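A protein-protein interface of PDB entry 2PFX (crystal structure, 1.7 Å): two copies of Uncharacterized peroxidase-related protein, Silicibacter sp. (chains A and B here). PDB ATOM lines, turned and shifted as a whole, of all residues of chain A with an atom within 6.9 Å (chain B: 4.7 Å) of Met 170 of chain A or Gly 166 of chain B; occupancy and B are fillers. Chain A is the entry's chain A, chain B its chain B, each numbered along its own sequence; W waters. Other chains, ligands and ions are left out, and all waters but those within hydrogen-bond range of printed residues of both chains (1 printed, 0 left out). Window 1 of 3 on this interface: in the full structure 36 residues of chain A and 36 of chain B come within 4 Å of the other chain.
OH of Tyr 44 of chain A sits at hydrogen-bond distance from OD1 of Asn 163 of chain B (2.6 Å).
The guanidinium group (NE) of Arg 173 of chain A is in hydrogen-bond range of the side-chain amide oxygen (OD1) of Asn 169 of chain B (3.4 Å).
The side-chain sulfur (SD) of Met 57 of chain A sits close to the side-chain sulfur (SD) of Met 57 of chain B (3.6 Å).
The side-chain sulfur (SD) of Met 57 of chain A sits close to the side-chain sulfur (SD) of Met 170 of chain B.
The side-chain sulfur of Met 57 of chain B lies close to the side-chain sulfur of Met 170 of chain A (3.7 Å).
The side-chain amide nitrogen (ND2) of Asn 84 of chain A lies within hydrogen-bond range of the side-chain amide oxygen (OD1) of Asn 169 of chain A, 3.3 Å away.
O of Thr 165 of chain A sits at hydrogen-bond distance from ND2 of Asn 169 of chain A.
OD1 of Asn 169 of chain A lies within hydrogen-bond range of NH1 of Arg 173 of chain A, 2.9 Å away.
The backbone carbonyl oxygen (O) of Thr 165 of chain B is in hydrogen-bond range of the side-chain amide nitrogen (ND2) of Asn 169 of chain B (2.9 Å).
Phe 54 of chain A touches Met 57 of chain B.
Met 170 of chain B touches Gly 166 of chain A (CB to O, 3.0 Å).
Phe 167 of chain A touches Met 170 of chain B.
Asn 169 of chain B touches Asn 169 of chain A.
O of Gly 166 of chain B touches CB of Met 170 of chain A (3.2 Å).
N of Phe 167 of chain B touches CG of Met 170 of chain A, at 3.7 Å.
Val 174 of chain A touches Ala 162 of chain B.
Val 174 of chain A touches Asn 163 of chain B.
Of the printed residues of chain B, Met 57 of chain A touches Met 57 (3.6 Å) and Met 170 (3.8 Å).
Met 170 of chain A touches three residues of chain B.
Phe 168 of chain B touches none of the printed residues of chain A.
Of the printed residues of chain A, Asn 169 of chain B touches Asn 169 (3.8 Å) and Arg 173 (3.3 Å).
Hydrophobic or aromatic side chains of chain A within 4 Å of the printed part of chain B: Tyr 44, Met 57, Met 170 and Val 174.
Among the printed residues, no Asp or Glu carboxylate lies within 4 Å of a Lys or Arg side-chain nitrogen of the other chain.
Met 57 of chain B touches its own counterpart, Met 57 of chain A.
Met 57 of chain A touches Met 170 of chain B, and with the chains exchanged Met 170 of chain A touches Met 57 of chain B.
Phe 167 of chain A touches Met 170 of chain B, and with the chains exchanged Met 170 of chain A touches Phe 167 of chain B.
Asn 169 of chain A touches its own counterpart, Asn 169 of chain B.
Positions printed for both chains: 57, 165, 166, 167, 168, 169 and 170.
Of the 13 pairs that touch across the chains among the printed residues, 8 have their exchanged pair printed and touching as well.
Water W1 bridges OD1 of Asn 169 of chain B (3.3 Å) and NH2 of Arg 173 of chain A (3.4 Å).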
ATOM      1  N   TYR A  44      -4.093  18.104   9.781  1.00  0.00           N
ATOM      2  CA  TYR A  44      -4.345  16.679   9.635  1.00  0.00           C
ATOM      3  C   TYR A  44      -5.265  16.128  10.709  1.00  0.00           C
ATOM      4  O   TYR A  44      -5.779  15.009  10.560  1.00  0.00           O
ATOM      5  CB  TYR A  44      -3.029  15.882   9.671  1.00  0.00           C
ATOM      6  CG  TYR A  44      -2.304  15.947   8.341  1.00  0.00           C
ATOM      7  CD1 TYR A  44      -1.414  16.977   8.089  1.00  0.00           C
ATOM      8  CD2 TYR A  44      -2.522  15.002   7.353  1.00  0.00           C
ATOM      9  CE1 TYR A  44      -0.760  17.043   6.871  1.00  0.00           C
ATOM     10  CE2 TYR A  44      -1.868  15.053   6.140  1.00  0.00           C
ATOM     11  CZ  TYR A  44      -0.989  16.079   5.914  1.00  0.00           C
ATOM     12  OH  TYR A  44      -0.328  16.150   4.714  1.00  0.00           O
ATOM     13  N   PHE A  54       0.935  10.838   8.933  1.00  0.00           N
ATOM     14  CA  PHE A  54       1.751  12.003   8.642  1.00  0.00           C
ATOM     15  C   PHE A  54       2.910  12.071   9.642  1.00  0.00           C
ATOM     16  O   PHE A  54       4.082  12.156   9.319  1.00  0.00           O
ATOM     17  CB  PHE A  54       0.922  13.297   8.701  1.00  0.00           C
ATOM     18  CG  PHE A  54       1.826  14.506   8.499  1.00  0.00           C
ATOM     19  CD1 PHE A  54       2.288  14.821   7.235  1.00  0.00           C
ATOM     20  CD2 PHE A  54       2.197  15.286   9.571  1.00  0.00           C
ATOM     21  CE1 PHE A  54       3.106  15.916   7.053  1.00  0.00           C
ATOM     22  CE2 PHE A  54       3.018  16.379   9.409  1.00  0.00           C
ATOM     23  CZ  PHE A  54       3.488  16.672   8.133  1.00  0.00           C
ATOM     24  N   MET A  57       5.643   9.351   9.630  1.00  0.00           N
ATOM     25  CA  MET A  57       6.644   9.567   8.603  1.00  0.00           C
ATOM     26  C   MET A  57       7.534  10.745   8.957  1.00  0.00           C
ATOM     27  O   MET A  57       8.752  10.607   8.862  1.00  0.00           O
ATOM     28  CB  MET A  57       5.951   9.790   7.258  1.00  0.00           C
ATOM     29  CG  MET A  57       6.975  10.032   6.162  1.00  0.00           C
ATOM     30  SD  MET A  57       6.276  10.026   4.397  1.00  0.00           S
ATOM     31  CE  MET A  57       5.893   8.141   4.416  1.00  0.00           C
ATOM     32  N   VAL A  80      14.850  22.765  -0.008  1.00  0.00           N
ATOM     33  CA  VAL A  80      13.690  22.320  -0.798  1.00  0.00           C
ATOM     34  C   VAL A  80      12.605  23.384  -0.757  1.00  0.00           C
ATOM     35  O   VAL A  80      12.107  23.795  -1.805  1.00  0.00           O
ATOM     36  CB  VAL A  80      13.155  20.958  -0.322  1.00  0.00           C
ATOM     37  CG1 VAL A  80      11.935  20.536  -1.133  1.00  0.00           C
ATOM     38  CG2 VAL A  80      14.244  19.895  -0.438  1.00  0.00           C
ATOM     39  N   ASN A  84      10.782  25.635  -3.804  1.00  0.00           N
ATOM     40  CA  ASN A  84       9.344  25.594  -4.049  1.00  0.00           C
ATOM     41  C   ASN A  84       8.582  26.806  -3.525  1.00  0.00           C
ATOM     42  O   ASN A  84       7.361  26.900  -3.763  1.00  0.00           O
ATOM     43  CB  ASN A  84       8.722  24.355  -3.403  1.00  0.00           C
ATOM     44  CG  ASN A  84       9.179  23.085  -4.097  1.00  0.00           C
ATOM     45  OD1 ASN A  84       9.388  23.062  -5.306  1.00  0.00           O
ATOM     46  ND2 ASN A  84       9.321  22.049  -3.314  1.00  0.00           N
ATOM     47  N   THR A 165      14.336  14.875   1.263  1.00  0.00           N
ATOM     48  CA  THR A 165      14.096  15.748   0.131  1.00  0.00           C
ATOM     49  C   THR A 165      12.710  15.505  -0.473  1.00  0.00           C
ATOM     50  O   THR A 165      11.904  16.421  -0.654  1.00  0.00           O
ATOM     51  CB  THR A 165      15.152  15.514  -0.974  1.00  0.00           C
ATOM     52  OG1 THR A 165      16.471  15.851  -0.493  1.00  0.00           O
ATOM     53  CG2 THR A 165      14.902  16.406  -2.176  1.00  0.00           C
ATOM     54  N   GLY A 166      12.390  14.251  -0.790  1.00  0.00           N
ATOM     55  CA  GLY A 166      11.081  13.918  -1.348  1.00  0.00           C
ATOM     56  C   GLY A 166       9.949  14.314  -0.420  1.00  0.00           C
ATOM     57  O   GLY A 166       8.934  14.845  -0.889  1.00  0.00           O
ATOM     58  N   PHE A 167      10.123  14.070   0.872  1.00  0.00           N
ATOM     59  CA  PHE A 167       9.086  14.428   1.845  1.00  0.00           C
ATOM     60  C   PHE A 167       8.761  15.910   1.782  1.00  0.00           C
ATOM     61  O   PHE A 167       7.573  16.222   1.774  1.00  0.00           O
ATOM     62  CB  PHE A 167       9.509  14.003   3.248  1.00  0.00           C
ATOM     63  CG  PHE A 167       8.494  14.198   4.351  1.00  0.00           C
ATOM     64  CD1 PHE A 167       7.319  13.475   4.431  1.00  0.00           C
ATOM     65  CD2 PHE A 167       8.767  15.153   5.318  1.00  0.00           C
ATOM     66  CE1 PHE A 167       6.433  13.710   5.466  1.00  0.00           C
ATOM     67  CE2 PHE A 167       7.921  15.384   6.373  1.00  0.00           C
ATOM     68  CZ  PHE A 167       6.763  14.635   6.437  1.00  0.00           C
ATOM     69  N   PHE A 168       9.740  16.820   1.711  1.00  0.00           N
ATOM     70  CA  PHE A 168       9.381  18.238   1.673  1.00  0.00           C
ATOM     71  C   PHE A 168       8.832  18.625   0.323  1.00  0.00           C
ATOM     72  O   PHE A 168       8.112  19.625   0.217  1.00  0.00           O
ATOM     73  CB  PHE A 168      10.568  19.137   2.104  1.00  0.00           C
ATOM     74  CG  PHE A 168      10.585  18.965   3.632  1.00  0.00           C
ATOM     75  CD1 PHE A 168       9.686  19.675   4.415  1.00  0.00           C
ATOM     76  CD2 PHE A 168      11.461  18.068   4.211  1.00  0.00           C
ATOM     77  CE1 PHE A 168       9.672  19.479   5.785  1.00  0.00           C
ATOM     78  CE2 PHE A 168      11.465  17.882   5.588  1.00  0.00           C
ATOM     79  CZ  PHE A 168      10.569  18.595   6.366  1.00  0.00           C
ATOM     80  N   ASN A 169       9.157  17.840  -0.709  1.00  0.00           N
ATOM     81  CA  ASN A 169       8.493  18.100  -1.990  1.00  0.00           C
ATOM     82  C   ASN A 169       6.995  17.749  -1.902  1.00  0.00           C
ATOM     83  O   ASN A 169       6.154  18.225  -2.684  1.00  0.00           O
ATOM     84  CB  ASN A 169       9.186  17.313  -3.107  1.00  0.00           C
ATOM     85  CG  ASN A 169      10.313  18.165  -3.685  1.00  0.00           C
ATOM     86  OD1 ASN A 169      10.036  19.073  -4.463  1.00  0.00           O
ATOM     87  ND2 ASN A 169      11.538  17.913  -3.272  1.00  0.00           N
ATOM     88  N   MET A 170       6.639  16.893  -0.948  1.00  0.00           N
ATOM     89  CA  MET A 170       5.234  16.574  -0.689  1.00  0.00           C
ATOM     90  C   MET A 170       4.651  17.705   0.169  1.00  0.00           C
ATOM     91  O   MET A 170       3.668  18.335  -0.203  1.00  0.00           O
ATOM     92  CB  MET A 170       4.994  15.251   0.012  1.00  0.00           C
ATOM     93  CG  MET A 170       3.589  15.051   0.598  1.00  0.00           C
ATOM     94  SD  MET A 170       3.416  13.289   1.390  1.00  0.00           S
ATOM     95  CE  MET A 170       4.221  13.897   3.029  1.00  0.00           C
ATOM     96  N   THR A 171       5.283  17.932   1.308  1.00  0.00           N
ATOM     97  CA  THR A 171       4.660  18.832   2.274  1.00  0.00           C
ATOM     98  C   THR A 171       4.632  20.245   1.753  1.00  0.00           C
ATOM     99  O   THR A 171       3.666  20.982   1.999  1.00  0.00           O
ATOM    100  CB  THR A 171       5.298  18.764   3.676  1.00  0.00           C
ATOM    101  OG1 THR A 171       6.622  19.280   3.694  1.00  0.00           O
ATOM    102  CG2 THR A 171       5.408  17.312   4.126  1.00  0.00           C
ATOM    103  N   ASN A 172       5.639  20.678   0.998  1.00  0.00           N
ATOM    104  CA  ASN A 172       5.533  22.010   0.405  1.00  0.00           C
ATOM    105  C   ASN A 172       4.291  22.156  -0.465  1.00  0.00           C
ATOM    106  O   ASN A 172       3.677  23.210  -0.401  1.00  0.00           O
ATOM    107  CB  ASN A 172       6.719  22.313  -0.488  1.00  0.00           C
ATOM    108  CG  ASN A 172       8.072  22.415   0.132  1.00  0.00           C
ATOM    109  OD1 ASN A 172       9.062  22.637  -0.563  1.00  0.00           O
ATOM    110  ND2 ASN A 172       8.082  22.184   1.428  1.00  0.00           N
ATOM    111  N   ARG A 173       4.001  21.112  -1.223  1.00  0.00           N
ATOM    112  CA  ARG A 173       2.903  21.184  -2.205  1.00  0.00           C
ATOM    113  C   ARG A 173       1.562  21.211  -1.507  1.00  0.00           C
ATOM    114  O   ARG A 173       0.640  21.949  -1.862  1.00  0.00           O
ATOM    115  CB  ARG A 173       3.056  20.021  -3.197  1.00  0.00           C
ATOM    116  CG  ARG A 173       4.249  20.285  -4.137  1.00  0.00           C
ATOM    117  CD  ARG A 173       4.414  19.263  -5.252  1.00  0.00           C
ATOM    118  NE  ARG A 173       5.309  19.856  -6.242  1.00  0.00           N
ATOM    119  CZ  ARG A 173       6.620  19.927  -6.235  1.00  0.00           C
ATOM    120  NH1 ARG A 173       7.304  19.397  -5.235  1.00  0.00           N
ATOM    121  NH2 ARG A 173       7.256  20.529  -7.232  1.00  0.00           N
ATOM    122  N   VAL A 174       1.472  20.360  -0.473  1.00  0.00           N
ATOM    123  CA  VAL A 174       0.224  20.344   0.288  1.00  0.00           C
ATOM    124  C   VAL A 174       0.008  21.684   0.964  1.00  0.00           C
ATOM    125  O   VAL A 174      -1.080  22.275   0.952  1.00  0.00           O
ATOM    126  CB  VAL A 174       0.285  19.193   1.301  1.00  0.00           C
ATOM    127  CG1 VAL A 174      -0.916  19.290   2.249  1.00  0.00           C
ATOM    128  CG2 VAL A 174       0.324  17.846   0.596  1.00  0.00           C
ATOM    129  N   ALA A 175       1.076  22.208   1.578  1.00  0.00           N
ATOM    130  CA  ALA A 175       0.922  23.455   2.319  1.00  0.00           C
ATOM    131  C   ALA A 175       0.554  24.594   1.388  1.00  0.00           C
ATOM    132  O   ALA A 175      -0.368  25.352   1.649  1.00  0.00           O
ATOM    133  CB  ALA A 175       2.188  23.786   3.110  1.00  0.00           C
ATOM    134  N   SER A 176       1.290  24.690   0.286  1.00  0.00           N
ATOM    135  CA  SER A 176       1.033  25.810  -0.620  1.00  0.00           C
ATOM    136  C   SER A 176      -0.327  25.634  -1.288  1.00  0.00           C
ATOM    137  O   SER A 176      -1.068  26.591  -1.468  1.00  0.00           O
ATOM    138  CB  SER A 176       2.151  25.962  -1.647  1.00  0.00           C
ATOM    139  OG  SER A 176       3.329  26.439  -1.030  1.00  0.00           O
ATOM    140  N   MET B  57       1.100   5.366   4.979  1.00  0.00           N
ATOM    141  CA  MET B  57       0.699   6.557   4.247  1.00  0.00           C
ATOM    142  C   MET B  57       0.169   6.177   2.867  1.00  0.00           C
ATOM    143  O   MET B  57      -0.863   6.704   2.476  1.00  0.00           O
ATOM    144  CB  MET B  57       1.855   7.552   4.122  1.00  0.00           C
ATOM    145  CG  MET B  57       1.436   8.814   3.366  1.00  0.00           C
ATOM    146  SD  MET B  57       2.827  10.150   3.296  1.00  0.00           S
ATOM    147  CE  MET B  57       2.417  10.696   5.107  1.00  0.00           C
ATOM    148  N   ALA B 162      -4.766  17.161  -3.000  1.00  0.00           N
ATOM    149  CA  ALA B 162      -3.496  17.783  -2.615  1.00  0.00           C
ATOM    150  C   ALA B 162      -2.557  16.753  -2.000  1.00  0.00           C
ATOM    151  O   ALA B 162      -1.365  16.732  -2.328  1.00  0.00           O
ATOM    152  CB  ALA B 162      -3.719  18.948  -1.676  1.00  0.00           C
ATOM    153  N   ASN B 163      -3.084  15.889  -1.143  1.00  0.00           N
ATOM    154  CA  ASN B 163      -2.156  14.922  -0.513  1.00  0.00           C
ATOM    155  C   ASN B 163      -1.705  13.836  -1.468  1.00  0.00           C
ATOM    156  O   ASN B 163      -0.541  13.407  -1.472  1.00  0.00           O
ATOM    157  CB  ASN B 163      -2.812  14.358   0.764  1.00  0.00           C
ATOM    158  CG  ASN B 163      -2.520  15.282   1.933  1.00  0.00           C
ATOM    159  OD1 ASN B 163      -1.550  15.078   2.666  1.00  0.00           O
ATOM    160  ND2 ASN B 163      -3.303  16.329   2.098  1.00  0.00           N
ATOM    161  N   VAL B 164      -2.592  13.343  -2.325  1.00  0.00           N
ATOM    162  CA  VAL B 164      -2.167  12.312  -3.273  1.00  0.00           C
ATOM    163  C   VAL B 164      -1.134  12.915  -4.199  1.00  0.00           C
ATOM    164  O   VAL B 164      -0.128  12.332  -4.556  1.00  0.00           O
ATOM    165  CB  VAL B 164      -3.371  11.789  -4.080  1.00  0.00           C
ATOM    166  CG1 VAL B 164      -2.912  10.902  -5.216  1.00  0.00           C
ATOM    167  CG2 VAL B 164      -4.318  11.027  -3.168  1.00  0.00           C
ATOM    168  N   THR B 165      -1.393  14.155  -4.653  1.00  0.00           N
ATOM    169  CA  THR B 165      -0.443  14.793  -5.549  1.00  0.00           C
ATOM    170  C   THR B 165       0.903  15.052  -4.867  1.00  0.00           C
ATOM    171  O   THR B 165       1.983  14.849  -5.443  1.00  0.00           O
ATOM    172  CB  THR B 165      -0.960  16.147  -6.042  1.00  0.00           C
ATOM    173  OG1 THR B 165      -2.198  16.017  -6.800  1.00  0.00           O
ATOM    174  CG2 THR B 165       0.086  16.823  -6.931  1.00  0.00           C
ATOM    175  N   GLY B 166       0.882  15.522  -3.614  1.00  0.00           N
ATOM    176  CA  GLY B 166       2.181  15.786  -2.960  1.00  0.00           C
ATOM    177  C   GLY B 166       2.888  14.453  -2.769  1.00  0.00           C
ATOM    178  O   GLY B 166       4.096  14.374  -2.946  1.00  0.00           O
ATOM    179  N   PHE B 167       2.162  13.394  -2.435  1.00  0.00           N
ATOM    180  CA  PHE B 167       2.795  12.102  -2.170  1.00  0.00           C
ATOM    181  C   PHE B 167       3.573  11.640  -3.391  1.00  0.00           C
ATOM    182  O   PHE B 167       4.704  11.180  -3.219  1.00  0.00           O
ATOM    183  CB  PHE B 167       1.755  11.093  -1.718  1.00  0.00           C
ATOM    184  CG  PHE B 167       2.223   9.688  -1.402  1.00  0.00           C
ATOM    185  CD1 PHE B 167       2.843   9.434  -0.184  1.00  0.00           C
ATOM    186  CD2 PHE B 167       2.035   8.668  -2.305  1.00  0.00           C
ATOM    187  CE1 PHE B 167       3.305   8.159   0.093  1.00  0.00           C
ATOM    188  CE2 PHE B 167       2.502   7.386  -2.045  1.00  0.00           C
ATOM    189  CZ  PHE B 167       3.126   7.145  -0.839  1.00  0.00           C
ATOM    190  N   PHE B 168       3.031  11.742  -4.602  1.00  0.00           N
ATOM    191  CA  PHE B 168       3.763  11.288  -5.780  1.00  0.00           C
ATOM    192  C   PHE B 168       4.878  12.252  -6.107  1.00  0.00           C
ATOM    193  O   PHE B 168       5.851  11.838  -6.753  1.00  0.00           O
ATOM    194  CB  PHE B 168       2.786  11.045  -6.959  1.00  0.00           C
ATOM    195  CG  PHE B 168       2.142   9.684  -6.622  1.00  0.00           C
ATOM    196  CD1 PHE B 168       2.849   8.504  -6.839  1.00  0.00           C
ATOM    197  CD2 PHE B 168       0.884   9.640  -6.048  1.00  0.00           C
ATOM    198  CE1 PHE B 168       2.312   7.271  -6.472  1.00  0.00           C
ATOM    199  CE2 PHE B 168       0.352   8.417  -5.687  1.00  0.00           C
ATOM    200  CZ  PHE B 168       1.063   7.262  -5.863  1.00  0.00           C
ATOM    201  N   ASN B 169       4.762  13.506  -5.645  1.00  0.00           N
ATOM    202  CA  ASN B 169       5.931  14.383  -5.813  1.00  0.00           C
ATOM    203  C   ASN B 169       7.091  13.916  -4.929  1.00  0.00           C
ATOM    204  O   ASN B 169       8.261  14.178  -5.254  1.00  0.00           O
ATOM    205  CB  ASN B 169       5.577  15.854  -5.576  1.00  0.00           C
ATOM    206  CG  ASN B 169       5.082  16.435  -6.895  1.00  0.00           C
ATOM    207  OD1 ASN B 169       5.885  16.820  -7.733  1.00  0.00           O
ATOM    208  ND2 ASN B 169       3.764  16.470  -7.096  1.00  0.00           N
ATOM    209  N   MET B 170       6.801  13.207  -3.842  1.00  0.00           N
ATOM    210  CA  MET B 170       7.855  12.629  -3.002  1.00  0.00           C
ATOM    211  C   MET B 170       8.349  11.340  -3.653  1.00  0.00           C
ATOM    212  O   MET B 170       9.533  11.190  -3.917  1.00  0.00           O
ATOM    213  CB  MET B 170       7.420  12.351  -1.576  1.00  0.00           C
ATOM    214  CG  MET B 170       8.187  11.303  -0.783  1.00  0.00           C
ATOM    215  SD  MET B 170       7.511  11.061   1.008  1.00  0.00           S
ATOM    216  CE  MET B 170       6.036  10.003   0.380  1.00  0.00           C
HETATM  217  O   HOH W   1       7.724  18.535  -9.901  1.00  0.00           O
